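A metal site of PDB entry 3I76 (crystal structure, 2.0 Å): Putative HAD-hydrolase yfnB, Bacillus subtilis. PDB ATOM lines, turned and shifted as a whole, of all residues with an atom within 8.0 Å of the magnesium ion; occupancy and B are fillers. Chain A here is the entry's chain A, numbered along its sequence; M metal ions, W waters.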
ATOM      1  N   PHE A  11       0.325 -29.342   9.170  1.00  0.00           N
ATOM      2  CA  PHE A  11      -1.110 -29.416   9.471  1.00  0.00           C
ATOM      3  C   PHE A  11      -1.364 -29.598  10.949  1.00  0.00           C
ATOM      4  O   PHE A  11      -0.844 -30.501  11.572  1.00  0.00           O
ATOM      5  CB  PHE A  11      -1.793 -30.560   8.737  1.00  0.00           C
ATOM      6  CG  PHE A  11      -2.051 -30.290   7.268  1.00  0.00           C
ATOM      7  CD1 PHE A  11      -3.282 -29.826   6.833  1.00  0.00           C
ATOM      8  CD2 PHE A  11      -1.088 -30.556   6.330  1.00  0.00           C
ATOM      9  CE1 PHE A  11      -3.534 -29.595   5.497  1.00  0.00           C
ATOM     10  CE2 PHE A  11      -1.327 -30.337   4.978  1.00  0.00           C
ATOM     11  CZ  PHE A  11      -2.539 -29.847   4.552  1.00  0.00           C
ATOM     12  N   ASP A  12      -2.201 -28.733  11.495  1.00  0.00           N
ATOM     13  CA  ASP A  12      -2.931 -29.048  12.683  1.00  0.00           C
ATOM     14  C   ASP A  12      -3.803 -30.283  12.457  1.00  0.00           C
ATOM     15  O   ASP A  12      -4.184 -30.618  11.323  1.00  0.00           O
ATOM     16  CB  ASP A  12      -3.801 -27.840  13.077  1.00  0.00           C
ATOM     17  CG  ASP A  12      -4.574 -28.075  14.338  1.00  0.00           C
ATOM     18  OD1 ASP A  12      -3.967 -28.477  15.343  1.00  0.00           O
ATOM     19  OD2 ASP A  12      -5.816 -27.898  14.344  1.00  0.00           O
ATOM     20  N   VAL A  13      -4.120 -30.966  13.550  1.00  0.00           N
ATOM     21  CA  VAL A  13      -5.034 -32.090  13.507  1.00  0.00           C
ATOM     22  C   VAL A  13      -6.476 -31.702  13.797  1.00  0.00           C
ATOM     23  O   VAL A  13      -7.320 -31.799  12.918  1.00  0.00           O
ATOM     24  CB  VAL A  13      -4.633 -33.231  14.478  1.00  0.00           C
ATOM     25  CG1 VAL A  13      -5.679 -34.364  14.380  1.00  0.00           C
ATOM     26  CG2 VAL A  13      -3.216 -33.768  14.119  1.00  0.00           C
ATOM     27  N   ASP A  14      -6.759 -31.263  15.001  1.00  0.00           N
ATOM     28  CA  ASP A  14      -8.155 -31.198  15.474  1.00  0.00           C
ATOM     29  C   ASP A  14      -8.893 -29.947  14.991  1.00  0.00           C
ATOM     30  O   ASP A  14      -8.470 -28.803  15.233  1.00  0.00           O
ATOM     31  CB  ASP A  14      -8.214 -31.310  16.985  1.00  0.00           C
ATOM     32  CG  ASP A  14      -7.844 -32.698  17.473  1.00  0.00           C
ATOM     33  OD1 ASP A  14      -8.269 -33.693  16.824  1.00  0.00           O
ATOM     34  OD2 ASP A  14      -7.165 -32.784  18.540  1.00  0.00           O
ATOM     35  N   ASP A  15     -10.014 -30.200  14.304  1.00  0.00           N
ATOM     36  CA  ASP A  15     -10.801 -29.234  13.506  1.00  0.00           C
ATOM     37  C   ASP A  15     -10.082 -28.599  12.320  1.00  0.00           C
ATOM     38  O   ASP A  15     -10.525 -27.615  11.767  1.00  0.00           O
ATOM     39  CB  ASP A  15     -11.442 -28.222  14.426  1.00  0.00           C
ATOM     40  CG  ASP A  15     -12.430 -28.898  15.386  1.00  0.00           C
ATOM     41  OD1 ASP A  15     -13.121 -29.844  14.919  1.00  0.00           O
ATOM     42  OD2 ASP A  15     -12.494 -28.540  16.576  1.00  0.00           O
ATOM     43  N   THR A  16      -8.981 -29.236  11.896  1.00  0.00           N
ATOM     44  CA  THR A  16      -8.315 -28.906  10.626  1.00  0.00           C
ATOM     45  C   THR A  16      -8.460 -30.040   9.646  1.00  0.00           C
ATOM     46  O   THR A  16      -9.031 -29.841   8.568  1.00  0.00           O
ATOM     47  CB  THR A  16      -6.864 -28.543  10.844  1.00  0.00           C
ATOM     48  OG1 THR A  16      -6.803 -27.419  11.731  1.00  0.00           O
ATOM     49  CG2 THR A  16      -6.179 -28.191   9.510  1.00  0.00           C
ATOM     50  N   ILE A  17      -8.002 -31.249  10.010  1.00  0.00           N
ATOM     51  CA  ILE A  17      -8.230 -32.406   9.144  1.00  0.00           C
ATOM     52  C   ILE A  17      -9.103 -33.463   9.785  1.00  0.00           C
ATOM     53  O   ILE A  17      -9.691 -34.246   9.073  1.00  0.00           O
ATOM     54  CB  ILE A  17      -6.902 -33.018   8.629  1.00  0.00           C
ATOM     55  CG1 ILE A  17      -5.996 -33.423   9.796  1.00  0.00           C
ATOM     56  CG2 ILE A  17      -6.188 -31.981   7.736  1.00  0.00           C
ATOM     57  CD1 ILE A  17      -4.575 -33.878   9.396  1.00  0.00           C
ATOM     58  N   LEU A  18      -9.179 -33.501  11.112  1.00  0.00           N
ATOM     59  CA  LEU A  18     -10.090 -34.396  11.815  1.00  0.00           C
ATOM     60  C   LEU A  18     -11.178 -33.557  12.455  1.00  0.00           C
ATOM     61  O   LEU A  18     -10.915 -32.426  12.938  1.00  0.00           O
ATOM     62  CB  LEU A  18      -9.377 -35.220  12.887  1.00  0.00           C
ATOM     63  CG  LEU A  18      -8.352 -36.270  12.438  1.00  0.00           C
ATOM     64  CD1 LEU A  18      -7.885 -37.082  13.631  1.00  0.00           C
ATOM     65  CD2 LEU A  18      -8.997 -37.190  11.400  1.00  0.00           C
ATOM     66  N   PHE A  20     -12.934 -32.838  15.222  1.00  0.00           N
ATOM     67  CA  PHE A  20     -12.812 -32.973  16.672  1.00  0.00           C
ATOM     68  C   PHE A  20     -14.139 -32.615  17.364  1.00  0.00           C
ATOM     69  O   PHE A  20     -14.494 -33.214  18.388  1.00  0.00           O
ATOM     70  CB  PHE A  20     -11.602 -32.156  17.234  1.00  0.00           C
ATOM     71  CG  PHE A  20     -11.369 -32.363  18.716  1.00  0.00           C
ATOM     72  CD1 PHE A  20     -10.721 -33.508  19.166  1.00  0.00           C
ATOM     73  CD2 PHE A  20     -11.863 -31.462  19.643  1.00  0.00           C
ATOM     74  CE1 PHE A  20     -10.523 -33.726  20.519  1.00  0.00           C
ATOM     75  CE2 PHE A  20     -11.699 -31.676  21.020  1.00  0.00           C
ATOM     76  CZ  PHE A  20     -11.017 -32.792  21.466  1.00  0.00           C
ATOM     77  N   GLN A  21     -14.878 -31.663  16.795  1.00  0.00           N
ATOM     78  CA  GLN A  21     -16.158 -31.288  17.378  1.00  0.00           C
ATOM     79  C   GLN A  21     -17.069 -32.506  17.515  1.00  0.00           C
ATOM     80  O   GLN A  21     -17.712 -32.701  18.552  1.00  0.00           O
ATOM     81  CB  GLN A  21     -16.829 -30.211  16.548  1.00  0.00           C
ATOM     82  CG  GLN A  21     -16.082 -28.866  16.584  1.00  0.00           C
ATOM     83  CD  GLN A  21     -15.784 -28.432  17.988  1.00  0.00           C
ATOM     84  OE1 GLN A  21     -16.704 -28.144  18.769  1.00  0.00           O
ATOM     85  NE2 GLN A  21     -14.481 -28.388  18.359  1.00  0.00           N
ATOM     86  N   VAL A 123       1.495 -30.831  13.315  1.00  0.00           N
ATOM     87  CA  VAL A 123       1.833 -29.968  14.441  1.00  0.00           C
ATOM     88  C   VAL A 123       0.621 -29.880  15.357  1.00  0.00           C
ATOM     89  O   VAL A 123      -0.454 -29.421  14.971  1.00  0.00           O
ATOM     90  CB  VAL A 123       2.289 -28.579  13.989  1.00  0.00           C
ATOM     91  CG1 VAL A 123       3.763 -28.671  13.462  1.00  0.00           C
ATOM     92  CG2 VAL A 123       1.389 -28.005  12.875  1.00  0.00           C
ATOM     93  N   THR A 124       0.760 -30.380  16.564  1.00  0.00           N
ATOM     94  CA  THR A 124      -0.401 -30.524  17.464  1.00  0.00           C
ATOM     95  C   THR A 124      -0.015 -30.419  18.918  1.00  0.00           C
ATOM     96  O   THR A 124       1.055 -30.883  19.297  1.00  0.00           O
ATOM     97  CB  THR A 124      -1.084 -31.917  17.221  1.00  0.00           C
ATOM     98  OG1 THR A 124      -2.242 -32.051  18.050  1.00  0.00           O
ATOM     99  CG2 THR A 124      -0.151 -33.099  17.586  1.00  0.00           C
ATOM    100  N   ASN A 125      -0.880 -29.813  19.728  1.00  0.00           N
ATOM    101  CA  ASN A 125      -0.806 -29.829  21.177  1.00  0.00           C
ATOM    102  C   ASN A 125      -1.601 -30.972  21.828  1.00  0.00           C
ATOM    103  O   ASN A 125      -1.611 -31.104  23.045  1.00  0.00           O
ATOM    104  CB  ASN A 125      -1.320 -28.519  21.770  1.00  0.00           C
ATOM    105  CG  ASN A 125      -0.408 -27.319  21.466  1.00  0.00           C
ATOM    106  OD1 ASN A 125       0.703 -27.483  20.947  1.00  0.00           O
ATOM    107  ND2 ASN A 125      -0.905 -26.120  21.758  1.00  0.00           N
ATOM    108  N   GLN A 131      -3.837 -38.745  19.242  1.00  0.00           N
ATOM    109  CA  GLN A 131      -3.647 -38.247  17.886  1.00  0.00           C
ATOM    110  C   GLN A 131      -3.167 -39.364  16.950  1.00  0.00           C
ATOM    111  O   GLN A 131      -3.711 -39.514  15.866  1.00  0.00           O
ATOM    112  CB  GLN A 131      -2.699 -37.067  17.872  1.00  0.00           C
ATOM    113  CG  GLN A 131      -3.078 -35.901  18.824  1.00  0.00           C
ATOM    114  CD  GLN A 131      -4.479 -35.385  18.570  1.00  0.00           C
ATOM    115  OE1 GLN A 131      -5.443 -36.145  18.690  1.00  0.00           O
ATOM    116  NE2 GLN A 131      -4.595 -34.139  18.227  1.00  0.00           N
ATOM    117  N   LYS A 157       2.362 -25.056  20.866  1.00  0.00           N
ATOM    118  CA  LYS A 157       1.818 -24.007  20.006  1.00  0.00           C
ATOM    119  C   LYS A 157       1.096 -23.023  20.907  1.00  0.00           C
ATOM    120  O   LYS A 157       0.414 -23.447  21.815  1.00  0.00           O
ATOM    121  CB  LYS A 157       0.867 -24.536  18.946  1.00  0.00           C
ATOM    122  CG  LYS A 157       1.459 -25.502  17.935  1.00  0.00           C
ATOM    123  CD  LYS A 157       0.445 -25.823  16.814  1.00  0.00           C
ATOM    124  CE  LYS A 157      -0.833 -26.546  17.359  1.00  0.00           C
ATOM    125  NZ  LYS A 157      -1.752 -26.969  16.248  1.00  0.00           N
ATOM    126  N   ILE A 181      -1.275 -24.873   8.137  1.00  0.00           N
ATOM    127  CA  ILE A 181      -2.744 -24.903   7.961  1.00  0.00           C
ATOM    128  C   ILE A 181      -3.345 -25.308   9.318  1.00  0.00           C
ATOM    129  O   ILE A 181      -2.979 -26.329   9.886  1.00  0.00           O
ATOM    130  CB  ILE A 181      -3.200 -25.936   6.899  1.00  0.00           C
ATOM    131  CG1 ILE A 181      -2.543 -25.712   5.525  1.00  0.00           C
ATOM    132  CG2 ILE A 181      -4.721 -25.944   6.760  1.00  0.00           C
ATOM    133  CD1 ILE A 181      -1.256 -26.453   5.284  1.00  0.00           C
ATOM    134  N   GLY A 182      -4.255 -24.502   9.847  1.00  0.00           N
ATOM    135  CA  GLY A 182      -4.851 -24.811  11.138  1.00  0.00           C
ATOM    136  C   GLY A 182      -6.049 -23.905  11.432  1.00  0.00           C
ATOM    137  O   GLY A 182      -6.187 -22.863  10.790  1.00  0.00           O
ATOM    138  N   ASP A 183      -6.891 -24.329  12.374  1.00  0.00           N
ATOM    139  CA  ASP A 183      -8.133 -23.639  12.698  1.00  0.00           C
ATOM    140  C   ASP A 183      -7.977 -22.630  13.831  1.00  0.00           C
ATOM    141  O   ASP A 183      -8.854 -21.815  14.010  1.00  0.00           O
ATOM    142  CB  ASP A 183      -9.240 -24.669  13.090  1.00  0.00           C
ATOM    143  CG  ASP A 183      -8.907 -25.408  14.373  1.00  0.00           C
ATOM    144  OD1 ASP A 183      -7.844 -26.028  14.463  1.00  0.00           O
ATOM    145  OD2 ASP A 183      -9.666 -25.328  15.350  1.00  0.00           O
ATOM    146  N   SER A 184      -6.894 -22.711  14.610  1.00  0.00           N
ATOM    147  CA  SER A 184      -6.735 -21.842  15.780  1.00  0.00           C
ATOM    148  C   SER A 184      -5.999 -20.554  15.390  1.00  0.00           C
ATOM    149  O   SER A 184      -4.813 -20.587  15.007  1.00  0.00           O
ATOM    150  CB  SER A 184      -5.979 -22.504  16.898  1.00  0.00           C
ATOM    151  OG  SER A 184      -5.832 -21.583  17.975  1.00  0.00           O
ATOM    152  N   LEU A 185      -6.719 -19.434  15.514  1.00  0.00           N
ATOM    153  CA  LEU A 185      -6.186 -18.127  15.174  1.00  0.00           C
ATOM    154  C   LEU A 185      -4.980 -17.868  16.061  1.00  0.00           C
ATOM    155  O   LEU A 185      -3.974 -17.356  15.598  1.00  0.00           O
ATOM    156  CB  LEU A 185      -7.241 -17.024  15.437  1.00  0.00           C
ATOM    157  CG  LEU A 185      -7.511 -15.920  14.409  1.00  0.00           C
ATOM    158  CD1 LEU A 185      -8.476 -14.859  15.044  1.00  0.00           C
ATOM    159  CD2 LEU A 185      -6.240 -15.303  13.881  1.00  0.00           C
ATOM    160  N   ALA A 187      -3.232 -20.309  18.319  1.00  0.00           N
ATOM    161  CA  ALA A 187      -2.230 -21.398  18.313  1.00  0.00           C
ATOM    162  C   ALA A 187      -1.525 -21.638  16.980  1.00  0.00           C
ATOM    163  O   ALA A 187      -0.292 -21.843  16.974  1.00  0.00           O
ATOM    164  CB  ALA A 187      -2.884 -22.717  18.816  1.00  0.00           C
ATOM    165  N   ASP A 188      -2.278 -21.697  15.894  1.00  0.00           N
ATOM    166  CA  ASP A 188      -1.741 -22.042  14.582  1.00  0.00           C
ATOM    167  C   ASP A 188      -1.330 -20.843  13.747  1.00  0.00           C
ATOM    168  O   ASP A 188      -0.249 -20.830  13.138  1.00  0.00           O
ATOM    169  CB  ASP A 188      -2.771 -22.838  13.773  1.00  0.00           C
ATOM    170  CG  ASP A 188      -3.224 -24.094  14.491  1.00  0.00           C
ATOM    171  OD1 ASP A 188      -2.326 -24.806  14.995  1.00  0.00           O
ATOM    172  OD2 ASP A 188      -4.462 -24.343  14.572  1.00  0.00           O
ATOM    173  N   MET A 202      -8.079 -22.203   8.641  1.00  0.00           N
ATOM    174  CA  MET A 202      -9.289 -23.001   8.395  1.00  0.00           C
ATOM    175  C   MET A 202     -10.461 -22.480   9.257  1.00  0.00           C
ATOM    176  O   MET A 202     -10.503 -22.703  10.467  1.00  0.00           O
ATOM    177  CB  MET A 202      -9.005 -24.500   8.665  1.00  0.00           C
ATOM    178  CG  MET A 202     -10.216 -25.402   8.460  1.00  0.00           C
ATOM    179  SD  MET A 202     -10.855 -25.502   6.790  1.00  0.00           S
ATOM    180  CE  MET A 202     -12.022 -26.809   7.109  1.00  0.00           C
HETATM  181 MG    MG M   1      -7.048 -27.318  15.792  1.00  0.00          MG
HETATM  182  O   HOH W   1      -5.764 -25.831  16.275  1.00  0.00           O
HETATM  183  O   HOH W   2      -8.463 -26.625  17.107  1.00  0.00           O
HETATM  184  O   HOH W   3      -6.269 -28.334  17.287  1.00  0.00           O
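The side-chain carboxylate of Asp 12 lies close to the side-chain hydroxyl of Thr 16, at 2.8 Å.
OD1 of Asp 12 lies within salt-bridge range of NZ of Lys 157.
The backbone NH of Asp 12 sits at hydrogen-bond distance from the backbone carbonyl oxygen of Ile 181 (3.0 Å).
N of Asp 183 sits at hydrogen-bond distance from OG1 of Thr 16 (3.2 Å).
N of Asp 183 is in hydrogen-bond range of OD2 of Asp 188 (3.3 Å).
NE2 of Gln 131 sits at hydrogen-bond distance from OD2 of Asp 14, 2.9 Å away.
Within 4 Å of the magnesium ion: Asp 12, Asp 14 and Asp 183.
Water W3 is bound to the magnesium ion, at 2.0 Å.
OD2 of Asp 12 is bound to the magnesium ion.
OD1 of Asp 183 binds the magnesium ion, 2.0 Å away.
Water W1 is bound to the magnesium ion, at 2.0 Å.
The magnesium ion is bound by water W2 (2.1 Å).
The backbone carbonyl oxygen (O) of Asp 14 is bound to the magnesium ion, 2.1 Å away.
The magnesium ion has six donor atoms within binding distance.
Water W1 bridges OD2 of Asp 188 (2.6 Å) and OD1 of Asp 12 (3.3 Å).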
